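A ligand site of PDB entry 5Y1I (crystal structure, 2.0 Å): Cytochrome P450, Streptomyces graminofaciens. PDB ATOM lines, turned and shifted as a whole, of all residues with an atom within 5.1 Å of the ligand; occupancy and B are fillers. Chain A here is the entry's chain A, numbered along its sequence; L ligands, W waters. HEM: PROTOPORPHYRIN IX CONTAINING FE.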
ATOM      1  N   HIS A  64     -11.104  17.164 -10.730  1.00  0.00           N
ATOM      2  CA  HIS A  64     -11.385  15.825 -10.275  1.00  0.00           C
ATOM      3  C   HIS A  64     -12.920  15.603 -10.224  1.00  0.00           C
ATOM      4  O   HIS A  64     -13.389  14.734  -9.525  1.00  0.00           O
ATOM      5  CB  HIS A  64     -10.752  15.633  -8.872  1.00  0.00           C
ATOM      6  CG  HIS A  64     -10.627  14.196  -8.447  1.00  0.00           C
ATOM      7  ND1 HIS A  64     -11.194  13.149  -9.138  1.00  0.00           N
ATOM      8  CD2 HIS A  64      -9.989  13.630  -7.406  1.00  0.00           C
ATOM      9  CE1 HIS A  64     -10.907  12.000  -8.530  1.00  0.00           C
ATOM     10  NE2 HIS A  64     -10.161  12.272  -7.486  1.00  0.00           N
ATOM     11  N   PHE A  88     -15.777  13.757  -0.621  1.00  0.00           N
ATOM     12  CA  PHE A  88     -14.856  14.865  -0.916  1.00  0.00           C
ATOM     13  C   PHE A  88     -13.701  14.518  -1.877  1.00  0.00           C
ATOM     14  O   PHE A  88     -13.147  15.399  -2.538  1.00  0.00           O
ATOM     15  CB  PHE A  88     -14.302  15.485   0.388  1.00  0.00           C
ATOM     16  CG  PHE A  88     -13.049  14.817   0.952  1.00  0.00           C
ATOM     17  CD1 PHE A  88     -11.791  15.195   0.526  1.00  0.00           C
ATOM     18  CD2 PHE A  88     -13.114  13.881   1.978  1.00  0.00           C
ATOM     19  CE1 PHE A  88     -10.636  14.600   1.034  1.00  0.00           C
ATOM     20  CE2 PHE A  88     -11.958  13.298   2.521  1.00  0.00           C
ATOM     21  CZ  PHE A  88     -10.710  13.658   2.051  1.00  0.00           C
ATOM     22  N   ALA A  89     -13.316  13.250  -1.953  1.00  0.00           N
ATOM     23  CA  ALA A  89     -12.249  12.857  -2.882  1.00  0.00           C
ATOM     24  C   ALA A  89     -12.587  13.034  -4.384  1.00  0.00           C
ATOM     25  O   ALA A  89     -11.672  13.026  -5.232  1.00  0.00           O
ATOM     26  CB  ALA A  89     -11.841  11.400  -2.596  1.00  0.00           C
ATOM     27  N   HIS A  96     -13.845  20.429  -1.720  1.00  0.00           N
ATOM     28  CA  HIS A  96     -12.851  19.380  -1.434  1.00  0.00           C
ATOM     29  C   HIS A  96     -12.033  19.767  -0.248  1.00  0.00           C
ATOM     30  O   HIS A  96     -11.959  19.025   0.751  1.00  0.00           O
ATOM     31  CB  HIS A  96     -11.972  19.104  -2.670  1.00  0.00           C
ATOM     32  CG  HIS A  96     -10.682  18.449  -2.335  1.00  0.00           C
ATOM     33  ND1 HIS A  96      -9.499  19.150  -2.200  1.00  0.00           N
ATOM     34  CD2 HIS A  96     -10.383  17.148  -2.093  1.00  0.00           C
ATOM     35  CE1 HIS A  96      -8.532  18.312  -1.887  1.00  0.00           C
ATOM     36  NE2 HIS A  96      -9.047  17.098  -1.786  1.00  0.00           N
ATOM     37  N   ARG A 100     -11.713  18.208   3.511  1.00  0.00           N
ATOM     38  CA  ARG A 100     -10.419  17.586   3.831  1.00  0.00           C
ATOM     39  C   ARG A 100      -9.845  18.212   5.086  1.00  0.00           C
ATOM     40  O   ARG A 100      -9.216  17.517   5.893  1.00  0.00           O
ATOM     41  CB  ARG A 100      -9.433  17.736   2.656  1.00  0.00           C
ATOM     42  CG  ARG A 100      -8.046  17.206   2.963  1.00  0.00           C
ATOM     43  CD  ARG A 100      -7.347  16.676   1.712  1.00  0.00           C
ATOM     44  NE  ARG A 100      -5.940  16.381   1.969  1.00  0.00           N
ATOM     45  CZ  ARG A 100      -5.153  15.546   1.269  1.00  0.00           C
ATOM     46  NH1 ARG A 100      -5.570  14.823   0.261  1.00  0.00           N
ATOM     47  NH2 ARG A 100      -3.948  15.398   1.655  1.00  0.00           N
ATOM     48  N   PHE A 107      -4.038  12.867  10.612  1.00  0.00           N
ATOM     49  CA  PHE A 107      -3.135  12.234   9.655  1.00  0.00           C
ATOM     50  C   PHE A 107      -1.794  12.902   9.518  1.00  0.00           C
ATOM     51  O   PHE A 107      -0.938  12.440   8.759  1.00  0.00           O
ATOM     52  CB  PHE A 107      -3.824  12.118   8.289  1.00  0.00           C
ATOM     53  CG  PHE A 107      -4.976  11.123   8.303  1.00  0.00           C
ATOM     54  CD1 PHE A 107      -4.748   9.754   8.085  1.00  0.00           C
ATOM     55  CD2 PHE A 107      -6.275  11.549   8.560  1.00  0.00           C
ATOM     56  CE1 PHE A 107      -5.822   8.853   8.158  1.00  0.00           C
ATOM     57  CE2 PHE A 107      -7.296  10.646   8.657  1.00  0.00           C
ATOM     58  CZ  PHE A 107      -7.086   9.304   8.442  1.00  0.00           C
ATOM     59  N   ILE A 152      -7.440   1.763  11.139  1.00  0.00           N
ATOM     60  CA  ILE A 152      -8.384   2.823  10.826  1.00  0.00           C
ATOM     61  C   ILE A 152      -9.545   2.824  11.817  1.00  0.00           C
ATOM     62  O   ILE A 152      -9.978   3.893  12.246  1.00  0.00           O
ATOM     63  CB  ILE A 152      -8.929   2.759   9.419  1.00  0.00           C
ATOM     64  CG1 ILE A 152      -7.811   2.840   8.409  1.00  0.00           C
ATOM     65  CG2 ILE A 152      -9.787   3.982   9.157  1.00  0.00           C
ATOM     66  CD1 ILE A 152      -8.266   2.482   7.009  1.00  0.00           C
ATOM     67  N   MET A 233     -15.638   6.681   3.694  1.00  0.00           N
ATOM     68  CA  MET A 233     -14.625   6.908   2.734  1.00  0.00           C
ATOM     69  C   MET A 233     -13.207   6.655   3.280  1.00  0.00           C
ATOM     70  O   MET A 233     -12.333   6.107   2.604  1.00  0.00           O
ATOM     71  CB  MET A 233     -14.840   8.309   2.224  1.00  0.00           C
ATOM     72  CG  MET A 233     -13.973   8.637   1.058  1.00  0.00           C
ATOM     73  SD  MET A 233     -12.496   9.544   1.482  1.00  0.00           S
ATOM     74  CE  MET A 233     -12.903  10.316   3.042  1.00  0.00           C
ATOM     75  N   LEU A 234     -12.956   7.048   4.511  1.00  0.00           N
ATOM     76  CA  LEU A 234     -11.659   6.790   5.122  1.00  0.00           C
ATOM     77  C   LEU A 234     -11.471   5.296   5.337  1.00  0.00           C
ATOM     78  O   LEU A 234     -10.443   4.758   4.978  1.00  0.00           O
ATOM     79  CB  LEU A 234     -11.535   7.511   6.433  1.00  0.00           C
ATOM     80  CG  LEU A 234     -11.515   9.016   6.352  1.00  0.00           C
ATOM     81  CD1 LEU A 234     -11.550   9.537   7.761  1.00  0.00           C
ATOM     82  CD2 LEU A 234     -10.297   9.515   5.653  1.00  0.00           C
ATOM     83  N   ALA A 237     -10.824   3.801   1.668  1.00  0.00           N
ATOM     84  CA  ALA A 237      -9.570   4.304   1.131  1.00  0.00           C
ATOM     85  C   ALA A 237      -8.315   3.699   1.709  1.00  0.00           C
ATOM     86  O   ALA A 237      -7.312   3.479   0.997  1.00  0.00           O
ATOM     87  CB  ALA A 237      -9.520   5.798   1.298  1.00  0.00           C
ATOM     88  N   GLY A 238      -8.368   3.447   3.010  1.00  0.00           N
ATOM     89  CA  GLY A 238      -7.220   3.055   3.720  1.00  0.00           C
ATOM     90  C   GLY A 238      -7.038   1.561   3.850  1.00  0.00           C
ATOM     91  O   GLY A 238      -6.024   1.127   4.425  1.00  0.00           O
ATOM     92  N   THR A 241      -5.830  -0.803  -0.379  1.00  0.00           N
ATOM     93  CA  THR A 241      -4.548  -0.293  -0.826  1.00  0.00           C
ATOM     94  C   THR A 241      -3.438  -0.747   0.080  1.00  0.00           C
ATOM     95  O   THR A 241      -2.447  -1.299  -0.379  1.00  0.00           O
ATOM     96  CB  THR A 241      -4.560   1.253  -0.821  1.00  0.00           C
ATOM     97  OG1 THR A 241      -5.147   1.721   0.418  1.00  0.00           O
ATOM     98  CG2 THR A 241      -5.385   1.805  -2.004  1.00  0.00           C
ATOM     99  N   THR A 242      -3.600  -0.514   1.370  1.00  0.00           N
ATOM    100  CA  THR A 242      -2.589  -0.826   2.345  1.00  0.00           C
ATOM    101  C   THR A 242      -2.378  -2.332   2.418  1.00  0.00           C
ATOM    102  O   THR A 242      -1.237  -2.824   2.475  1.00  0.00           O
ATOM    103  CB  THR A 242      -2.919  -0.309   3.730  1.00  0.00           C
ATOM    104  OG1 THR A 242      -3.270   1.065   3.667  1.00  0.00           O
ATOM    105  CG2 THR A 242      -1.725  -0.426   4.607  1.00  0.00           C
ATOM    106  N   MET A 245      -0.329  -3.501  -0.456  1.00  0.00           N
ATOM    107  CA  MET A 245       1.068  -3.173  -0.203  1.00  0.00           C
ATOM    108  C   MET A 245       1.716  -4.190   0.773  1.00  0.00           C
ATOM    109  O   MET A 245       2.856  -4.643   0.567  1.00  0.00           O
ATOM    110  CB  MET A 245       1.276  -1.758   0.313  1.00  0.00           C
ATOM    111  CG  MET A 245       1.292  -0.662  -0.778  1.00  0.00           C
ATOM    112  SD  MET A 245       2.527  -1.024  -2.076  1.00  0.00           S
ATOM    113  CE  MET A 245       4.012  -0.768  -1.131  1.00  0.00           C
ATOM    114  N   LEU A 280       6.906   1.107  -2.371  1.00  0.00           N
ATOM    115  CA  LEU A 280       5.828   1.919  -2.900  1.00  0.00           C
ATOM    116  C   LEU A 280       6.083   2.249  -4.376  1.00  0.00           C
ATOM    117  O   LEU A 280       5.184   2.092  -5.207  1.00  0.00           O
ATOM    118  CB  LEU A 280       5.656   3.197  -2.070  1.00  0.00           C
ATOM    119  CG  LEU A 280       5.065   2.919  -0.699  1.00  0.00           C
ATOM    120  CD1 LEU A 280       5.308   4.086   0.237  1.00  0.00           C
ATOM    121  CD2 LEU A 280       3.578   2.690  -0.830  1.00  0.00           C
ATOM    122  N   ILE A 285       0.945   0.196  -6.532  1.00  0.00           N
ATOM    123  CA  ILE A 285      -0.324  -0.537  -6.577  1.00  0.00           C
ATOM    124  C   ILE A 285      -1.531   0.318  -6.973  1.00  0.00           C
ATOM    125  O   ILE A 285      -2.510  -0.217  -7.481  1.00  0.00           O
ATOM    126  CB  ILE A 285      -0.607  -1.318  -5.262  1.00  0.00           C
ATOM    127  CG1 ILE A 285      -0.718  -0.433  -4.034  1.00  0.00           C
ATOM    128  CG2 ILE A 285       0.545  -2.277  -5.045  1.00  0.00           C
ATOM    129  CD1 ILE A 285      -2.103   0.158  -3.793  1.00  0.00           C
ATOM    130  N   ALA A 286      -1.446   1.632  -6.839  1.00  0.00           N
ATOM    131  CA  ALA A 286      -2.597   2.455  -7.262  1.00  0.00           C
ATOM    132  C   ALA A 286      -2.653   2.615  -8.806  1.00  0.00           C
ATOM    133  O   ALA A 286      -3.638   3.105  -9.335  1.00  0.00           O
ATOM    134  CB  ALA A 286      -2.564   3.784  -6.561  1.00  0.00           C
ATOM    135  N   THR A 289      -5.320   4.478 -11.289  1.00  0.00           N
ATOM    136  CA  THR A 289      -6.533   4.869 -10.624  1.00  0.00           C
ATOM    137  C   THR A 289      -6.734   6.376 -10.504  1.00  0.00           C
ATOM    138  O   THR A 289      -7.789   6.838 -10.055  1.00  0.00           O
ATOM    139  CB  THR A 289      -6.656   4.247  -9.220  1.00  0.00           C
ATOM    140  OG1 THR A 289      -5.518   4.511  -8.386  1.00  0.00           O
ATOM    141  CG2 THR A 289      -6.796   2.774  -9.327  1.00  0.00           C
ATOM    142  N   VAL A 290      -5.699   7.144 -10.834  1.00  0.00           N
ATOM    143  CA  VAL A 290      -5.742   8.578 -10.778  1.00  0.00           C
ATOM    144  C   VAL A 290      -6.271   9.135 -12.111  1.00  0.00           C
ATOM    145  O   VAL A 290      -5.706   8.918 -13.196  1.00  0.00           O
ATOM    146  CB  VAL A 290      -4.379   9.142 -10.370  1.00  0.00           C
ATOM    147  CG1 VAL A 290      -4.316  10.634 -10.557  1.00  0.00           C
ATOM    148  CG2 VAL A 290      -4.082   8.740  -8.948  1.00  0.00           C
ATOM    149  N   ARG A 291      -7.404   9.830 -12.015  1.00  0.00           N
ATOM    150  CA  ARG A 291      -8.114  10.268 -13.180  1.00  0.00           C
ATOM    151  C   ARG A 291      -8.506  11.685 -13.000  1.00  0.00           C
ATOM    152  O   ARG A 291      -8.947  12.046 -11.948  1.00  0.00           O
ATOM    153  CB  ARG A 291      -9.373   9.446 -13.380  1.00  0.00           C
ATOM    154  CG  ARG A 291      -9.162   7.945 -13.491  1.00  0.00           C
ATOM    155  CD  ARG A 291      -8.497   7.601 -14.817  1.00  0.00           C
ATOM    156  NE  ARG A 291      -8.081   6.208 -14.912  1.00  0.00           N
ATOM    157  CZ  ARG A 291      -8.676   5.269 -15.655  1.00  0.00           C
ATOM    158  NH1 ARG A 291      -9.787   5.520 -16.346  1.00  0.00           N
ATOM    159  NH2 ARG A 291      -8.174   4.040 -15.678  1.00  0.00           N
ATOM    160  N   ARG A 292      -8.405  12.478 -14.083  1.00  0.00           N
ATOM    161  CA  ARG A 292      -8.909  13.821 -14.077  1.00  0.00           C
ATOM    162  C   ARG A 292      -9.582  14.172 -15.428  1.00  0.00           C
ATOM    163  O   ARG A 292      -9.555  13.376 -16.407  1.00  0.00           O
ATOM    164  CB  ARG A 292      -7.757  14.764 -13.841  1.00  0.00           C
ATOM    165  CG  ARG A 292      -6.965  14.531 -12.594  1.00  0.00           C
ATOM    166  CD  ARG A 292      -7.695  14.983 -11.339  1.00  0.00           C
ATOM    167  NE  ARG A 292      -6.819  14.897 -10.153  1.00  0.00           N
ATOM    168  CZ  ARG A 292      -6.713  13.872  -9.319  1.00  0.00           C
ATOM    169  NH1 ARG A 292      -7.343  12.744  -9.527  1.00  0.00           N
ATOM    170  NH2 ARG A 292      -5.942  13.986  -8.256  1.00  0.00           N
ATOM    171  N   LEU A 315       0.358   6.009 -12.601  1.00  0.00           N
ATOM    172  CA  LEU A 315       1.393   6.309 -11.602  1.00  0.00           C
ATOM    173  C   LEU A 315       2.575   5.337 -11.715  1.00  0.00           C
ATOM    174  O   LEU A 315       3.718   5.689 -11.353  1.00  0.00           O
ATOM    175  CB  LEU A 315       0.805   6.206 -10.201  1.00  0.00           C
ATOM    176  CG  LEU A 315      -0.389   7.169  -9.944  1.00  0.00           C
ATOM    177  CD1 LEU A 315      -0.991   6.975  -8.538  1.00  0.00           C
ATOM    178  CD2 LEU A 315       0.077   8.583 -10.068  1.00  0.00           C
ATOM    179  N   ALA A 344       3.398   7.205  -5.880  1.00  0.00           N
ATOM    180  CA  ALA A 344       2.515   6.137  -5.447  1.00  0.00           C
ATOM    181  C   ALA A 344       1.272   6.631  -4.682  1.00  0.00           C
ATOM    182  O   ALA A 344       0.266   5.951  -4.702  1.00  0.00           O
ATOM    183  CB  ALA A 344       3.238   5.132  -4.605  1.00  0.00           C
ATOM    184  N   PHE A 345       1.398   7.774  -4.025  1.00  0.00           N
ATOM    185  CA  PHE A 345       0.261   8.425  -3.317  1.00  0.00           C
ATOM    186  C   PHE A 345      -0.331   9.572  -4.097  1.00  0.00           C
ATOM    187  O   PHE A 345      -1.125  10.417  -3.577  1.00  0.00           O
ATOM    188  CB  PHE A 345       0.779   8.982  -2.014  1.00  0.00           C
ATOM    189  CG  PHE A 345       1.286   7.943  -1.112  1.00  0.00           C
ATOM    190  CD1 PHE A 345       0.440   6.949  -0.642  1.00  0.00           C
ATOM    191  CD2 PHE A 345       2.533   8.009  -0.603  1.00  0.00           C
ATOM    192  CE1 PHE A 345       0.886   6.006   0.239  1.00  0.00           C
ATOM    193  CE2 PHE A 345       2.993   7.055   0.292  1.00  0.00           C
ATOM    194  CZ  PHE A 345       2.167   6.068   0.712  1.00  0.00           C
ATOM    195  N   GLY A 346      -0.022   9.554  -5.380  1.00  0.00           N
ATOM    196  CA  GLY A 346      -0.484  10.608  -6.296  1.00  0.00           C
ATOM    197  C   GLY A 346       0.242  11.915  -6.070  1.00  0.00           C
ATOM    198  O   GLY A 346       1.379  11.947  -5.639  1.00  0.00           O
ATOM    199  N   VAL A 349      -3.390  18.516  -4.818  1.00  0.00           N
ATOM    200  CA  VAL A 349      -4.293  18.642  -3.663  1.00  0.00           C
ATOM    201  C   VAL A 349      -5.025  17.357  -3.249  1.00  0.00           C
ATOM    202  O   VAL A 349      -5.553  17.271  -2.117  1.00  0.00           O
ATOM    203  CB  VAL A 349      -5.306  19.786  -3.844  1.00  0.00           C
ATOM    204  CG1 VAL A 349      -4.559  21.095  -4.062  1.00  0.00           C
ATOM    205  CG2 VAL A 349      -6.229  19.494  -5.003  1.00  0.00           C
ATOM    206  N   HIS A 350      -5.071  16.357  -4.119  1.00  0.00           N
ATOM    207  CA  HIS A 350      -5.692  15.110  -3.758  1.00  0.00           C
ATOM    208  C   HIS A 350      -4.673  14.060  -3.350  1.00  0.00           C
ATOM    209  O   HIS A 350      -5.019  12.884  -3.172  1.00  0.00           O
ATOM    210  CB  HIS A 350      -6.547  14.578  -4.878  1.00  0.00           C
ATOM    211  CG  HIS A 350      -7.667  15.479  -5.283  1.00  0.00           C
ATOM    212  ND1 HIS A 350      -8.866  15.521  -4.596  1.00  0.00           N
ATOM    213  CD2 HIS A 350      -7.810  16.308  -6.356  1.00  0.00           C
ATOM    214  CE1 HIS A 350      -9.665  16.407  -5.177  1.00  0.00           C
ATOM    215  NE2 HIS A 350      -9.049  16.894  -6.247  1.00  0.00           N
ATOM    216  N   GLN A 351      -3.437  14.468  -3.227  1.00  0.00           N
ATOM    217  CA  GLN A 351      -2.427  13.515  -2.772  1.00  0.00           C
ATOM    218  C   GLN A 351      -2.932  12.723  -1.541  1.00  0.00           C
ATOM    219  O   GLN A 351      -3.509  13.307  -0.627  1.00  0.00           O
ATOM    220  CB  GLN A 351      -1.129  14.201  -2.432  1.00  0.00           C
ATOM    221  CG  GLN A 351       0.060  13.220  -2.343  1.00  0.00           C
ATOM    222  CD  GLN A 351       1.337  13.880  -1.827  1.00  0.00           C
ATOM    223  OE1 GLN A 351       1.303  14.704  -0.925  1.00  0.00           O
ATOM    224  NE2 GLN A 351       2.462  13.571  -2.440  1.00  0.00           N
ATOM    225  N   CYS A 352      -2.662  11.422  -1.529  1.00  0.00           N
ATOM    226  CA  CYS A 352      -3.091  10.541  -0.412  1.00  0.00           C
ATOM    227  C   CYS A 352      -3.063  11.188   0.982  1.00  0.00           C
ATOM    228  O   CYS A 352      -1.978  11.430   1.548  1.00  0.00           O
ATOM    229  CB  CYS A 352      -2.273   9.266  -0.299  1.00  0.00           C
ATOM    230  SG  CYS A 352      -3.112   8.081   0.788  1.00  0.00           S
ATOM    231  N   LEU A 353      -4.252  11.430   1.527  1.00  0.00           N
ATOM    232  CA  LEU A 353      -4.403  11.849   2.923  1.00  0.00           C
ATOM    233  C   LEU A 353      -3.718  10.905   3.935  1.00  0.00           C
ATOM    234  O   LEU A 353      -3.168  11.325   4.965  1.00  0.00           O
ATOM    235  CB  LEU A 353      -5.887  11.967   3.285  1.00  0.00           C
ATOM    236  CG  LEU A 353      -6.126  12.418   4.753  1.00  0.00           C
ATOM    237  CD1 LEU A 353      -5.545  13.765   5.062  1.00  0.00           C
ATOM    238  CD2 LEU A 353      -7.621  12.453   5.012  1.00  0.00           C
ATOM    239  N   GLY A 354      -3.769   9.621   3.643  1.00  0.00           N
ATOM    240  CA  GLY A 354      -3.175   8.628   4.535  1.00  0.00           C
ATOM    241  C   GLY A 354      -1.704   8.322   4.243  1.00  0.00           C
ATOM    242  O   GLY A 354      -1.217   7.340   4.697  1.00  0.00           O
ATOM    243  N   LEU A 357       0.456   7.745   7.362  1.00  0.00           N
ATOM    244  CA  LEU A 357      -0.062   6.572   8.030  1.00  0.00           C
ATOM    245  C   LEU A 357       0.361   5.271   7.311  1.00  0.00           C
ATOM    246  O   LEU A 357       0.855   4.330   7.946  1.00  0.00           O
ATOM    247  CB  LEU A 357      -1.564   6.679   8.124  1.00  0.00           C
ATOM    248  CG  LEU A 357      -2.223   5.458   8.679  1.00  0.00           C
ATOM    249  CD1 LEU A 357      -1.640   5.175  10.046  1.00  0.00           C
ATOM    250  CD2 LEU A 357      -3.741   5.701   8.723  1.00  0.00           C
ATOM    251  N   ALA A 358       0.218   5.256   5.986  1.00  0.00           N
ATOM    252  CA  ALA A 358       0.603   4.120   5.188  1.00  0.00           C
ATOM    253  C   ALA A 358       2.050   3.810   5.263  1.00  0.00           C
ATOM    254  O   ALA A 358       2.402   2.682   5.504  1.00  0.00           O
ATOM    255  CB  ALA A 358       0.143   4.242   3.772  1.00  0.00           C
ATOM    256  N   GLU A 361       2.547   2.397   8.828  1.00  0.00           N
ATOM    257  CA  GLU A 361       1.975   1.062   8.900  1.00  0.00           C
ATOM    258  C   GLU A 361       2.895   0.024   8.202  1.00  0.00           C
ATOM    259  O   GLU A 361       3.136  -0.992   8.738  1.00  0.00           O
ATOM    260  CB  GLU A 361       0.625   0.982   8.274  1.00  0.00           C
ATOM    261  CG  GLU A 361      -0.508   1.634   9.090  1.00  0.00           C
ATOM    262  CD  GLU A 361      -1.888   1.228   8.551  1.00  0.00           C
ATOM    263  OE1 GLU A 361      -2.126   0.014   8.322  1.00  0.00           O
ATOM    264  OE2 GLU A 361      -2.678   2.109   8.271  1.00  0.00           O
ATOM    265  N   LEU A 362       3.367   0.327   7.033  1.00  0.00           N
ATOM    266  CA  LEU A 362       4.162  -0.642   6.287  1.00  0.00           C
ATOM    267  C   LEU A 362       5.495  -0.813   6.938  1.00  0.00           C
ATOM    268  O   LEU A 362       5.997  -1.926   6.953  1.00  0.00           O
ATOM    269  CB  LEU A 362       4.333  -0.198   4.824  1.00  0.00           C
ATOM    270  CG  LEU A 362       3.039  -0.101   4.045  1.00  0.00           C
ATOM    271  CD1 LEU A 362       3.190   0.617   2.707  1.00  0.00           C
ATOM    272  CD2 LEU A 362       2.434  -1.472   3.880  1.00  0.00           C
HETATM  273  CHA HEM L   1      -6.016   9.482  -1.966  1.00  0.00           C
HETATM  274  CHB HEM L   1      -2.944   5.878  -2.686  1.00  0.00           C
HETATM  275  CHC HEM L   1      -3.332   4.536   1.949  1.00  0.00           C
HETATM  276  CHD HEM L   1      -6.819   7.738   2.388  1.00  0.00           C
HETATM  277  C1A HEM L   1      -5.113   8.666  -2.508  1.00  0.00           C
HETATM  278  C2A HEM L   1      -4.684   8.743  -3.835  1.00  0.00           C
HETATM  279  C3A HEM L   1      -3.800   7.717  -4.059  1.00  0.00           C
HETATM  280  C4A HEM L   1      -3.715   7.002  -2.851  1.00  0.00           C
HETATM  281  CMA HEM L   1      -3.045   7.421  -5.341  1.00  0.00           C
HETATM  282  CAA HEM L   1      -5.025   9.776  -4.853  1.00  0.00           C
HETATM  283  CBA HEM L   1      -6.329   9.517  -5.593  1.00  0.00           C
HETATM  284  CGA HEM L   1      -6.596  10.582  -6.598  1.00  0.00           C
HETATM  285  O1A HEM L   1      -5.820  11.515  -6.806  1.00  0.00           O
HETATM  286  O2A HEM L   1      -7.596  10.444  -7.312  1.00  0.00           O
HETATM  287  C1B HEM L   1      -2.791   5.186  -1.487  1.00  0.00           C
HETATM  288  C2B HEM L   1      -1.883   4.098  -1.276  1.00  0.00           C
HETATM  289  C3B HEM L   1      -1.981   3.729   0.036  1.00  0.00           C
HETATM  290  C4B HEM L   1      -2.966   4.610   0.612  1.00  0.00           C
HETATM  291  CMB HEM L   1      -0.993   3.521  -2.313  1.00  0.00           C
HETATM  292  CAB HEM L   1      -1.335   2.731   0.853  1.00  0.00           C
HETATM  293  CBB HEM L   1      -0.351   1.994   0.344  1.00  0.00           C
HETATM  294  C1C HEM L   1      -4.336   5.305   2.527  1.00  0.00           C
HETATM  295  C2C HEM L   1      -4.738   5.308   3.862  1.00  0.00           C
HETATM  296  C3C HEM L   1      -5.775   6.231   3.955  1.00  0.00           C
HETATM  297  C4C HEM L   1      -5.956   6.739   2.668  1.00  0.00           C
HETATM  298  CMC HEM L   1      -4.047   4.439   4.955  1.00  0.00           C
HETATM  299  CAC HEM L   1      -6.669   6.762   5.026  1.00  0.00           C
HETATM  300  CBC HEM L   1      -6.719   6.289   6.221  1.00  0.00           C
HETATM  301  C1D HEM L   1      -6.826   8.432   1.201  1.00  0.00           C
HETATM  302  C2D HEM L   1      -7.812   9.569   1.031  1.00  0.00           C
HETATM  303  C3D HEM L   1      -7.586  10.083  -0.207  1.00  0.00           C
HETATM  304  C4D HEM L   1      -6.502   9.218  -0.728  1.00  0.00           C
HETATM  305  CMD HEM L   1      -8.840  10.047   2.008  1.00  0.00           C
HETATM  306  CAD HEM L   1      -8.282  11.253  -0.857  1.00  0.00           C
HETATM  307  CBD HEM L   1      -7.492  12.542  -0.768  1.00  0.00           C
HETATM  308  CGD HEM L   1      -8.268  13.697  -1.415  1.00  0.00           C
HETATM  309  O1D HEM L   1      -8.953  13.555  -2.483  1.00  0.00           O
HETATM  310  O2D HEM L   1      -8.106  14.843  -0.923  1.00  0.00           O
HETATM  311  NA  HEM L   1      -4.537   7.547  -1.922  1.00  0.00           N
HETATM  312  NB  HEM L   1      -3.363   5.410  -0.376  1.00  0.00           N
HETATM  313  NC  HEM L   1      -5.019   6.199   1.841  1.00  0.00           N
HETATM  314  ND  HEM L   1      -6.087   8.285   0.156  1.00  0.00           N
HETATM  315 FE   HEM L   1      -4.735   6.926  -0.077  1.00  0.00          FE
HETATM  316  O   HOH W   1      -3.287  12.597  -6.377  1.00  0.00           O
HETATM  317  O   HOH W   2      -6.163   5.702  -0.865  1.00  0.00           O
HETATM  318  O   HOH W   3      -9.115  11.612  -4.708  1.00  0.00           O
HETATM  319  O   HOH W   4      -8.791   9.419  -9.479  1.00  0.00           O
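The backbone NH of Gly 354 sits close to the side-chain sulfur of Cys 352 (3.3 Å).
O of Ala 237 is in hydrogen-bond range of OG1 of Thr 241.
NH1 of Arg 100 sits at hydrogen-bond distance from O of Gln 351 (2.7 Å).
The backbone NH of Cys 352 sits at hydrogen-bond distance from the backbone carbonyl oxygen of Phe 345, at 2.8 Å.
O of Val 349 is in hydrogen-bond range of NH1 of Arg 100, at 3.4 Å.
The side-chain hydroxyl of Thr 289 lies within hydrogen-bond range of the backbone carbonyl oxygen of Ala 286, at 2.5 Å.
A ring nitrogen (ND1) of His 350 sits at hydrogen-bond distance from a ring nitrogen (NE2) of His 96 (3.2 Å).
The backbone carbonyl oxygen (O) of Gly 238 is in hydrogen-bond range of the side-chain hydroxyl (OG1) of Thr 242 (2.9 Å).
NE2 of His 96 is in hydrogen-bond range of O2D of the ligand (2.6 Å).
A ring nitrogen (NE2) of His 64 is in hydrogen-bond range of an oxygen (O2A) of the ligand (3.2 Å).
The guanidinium group (NH2) of Arg 292 lies within salt-bridge range of an oxygen (O1A) of the ligand (2.9 Å).
An iron atom (FE) of the ligand is bound by the side-chain sulfur of Cys 352, at 2.2 Å.
A ring nitrogen (ND1) of His 350 sits at hydrogen-bond distance from an oxygen (O1D) of the ligand (2.9 Å).
An oxygen (O2D) of the ligand is in salt-bridge range of the guanidinium group of Arg 100.
Water W4 lies within hydrogen-bond range of an oxygen (O2A) of the ligand, the backbone carbonyl oxygen (O) of Thr 289 and the backbone NH (N) of Arg 291.
Water W3 lies within hydrogen-bond range of an oxygen (O1D) of the ligand (3.0 Å), the backbone carbonyl oxygen (O) of Ala 89 (3.0 Å) and a ring nitrogen (NE2) of His 64 (3.0 Å).
CE1 of Phe 88 touches O2D of the ligand, 3.2 Å away.
CA of Ala 89 touches O1D of the ligand (3.4 Å).
Phe 107 touches the ligand.
Met 233 touches the ligand (SD to CMD, 3.7 Å).
Leu 234 touches the ligand (CD2 to CMD, 3.96 Å).
CB of Ala 237 touches CHD of the ligand (3.5 Å).
Gly 238 touches the ligand.
OG1 of Thr 241 touches C4B of the ligand, 3.6 Å away.
Thr 242 touches the ligand (OG1 to CMC, 3.7 Å).
CG of Met 245 touches CBB of the ligand (3.3 Å).
CD1 of Ile 285 touches CMB of the ligand, 3.8 Å away.
Ala 286 touches the ligand.
Val 290 touches the ligand.
Leu 315 touches the ligand.
O of Ala 344 touches CMB of the ligand (3.6 Å).
Phe 345 touches the ligand.
Gly 346 touches the ligand (N to CMA, 3.7 Å).
O of Val 349 touches O2D of the ligand (3.7 Å).
Leu 353 touches the ligand (CB to CMD, 3.7 Å).
Gly 354 touches the ligand.
Leu 357 touches the ligand.
Ala 358 touches the ligand.
Hydrophobic or aromatic side chains that line the ligand: His 64, Phe 88, Ala 89, His 96, Phe 107, Met 233, Leu 234, Ala 237, Met 245, Ile 285, Ala 286, Val 290, Leu 315, Phe 345, His 350, Leu 353, Leu 357 and Ala 358.
Of the 35 residues printed, 28 come within 4 Å of the ligand.
The nearest printed residue that does not touch the ligand is Gln 351 (4.1 Å).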
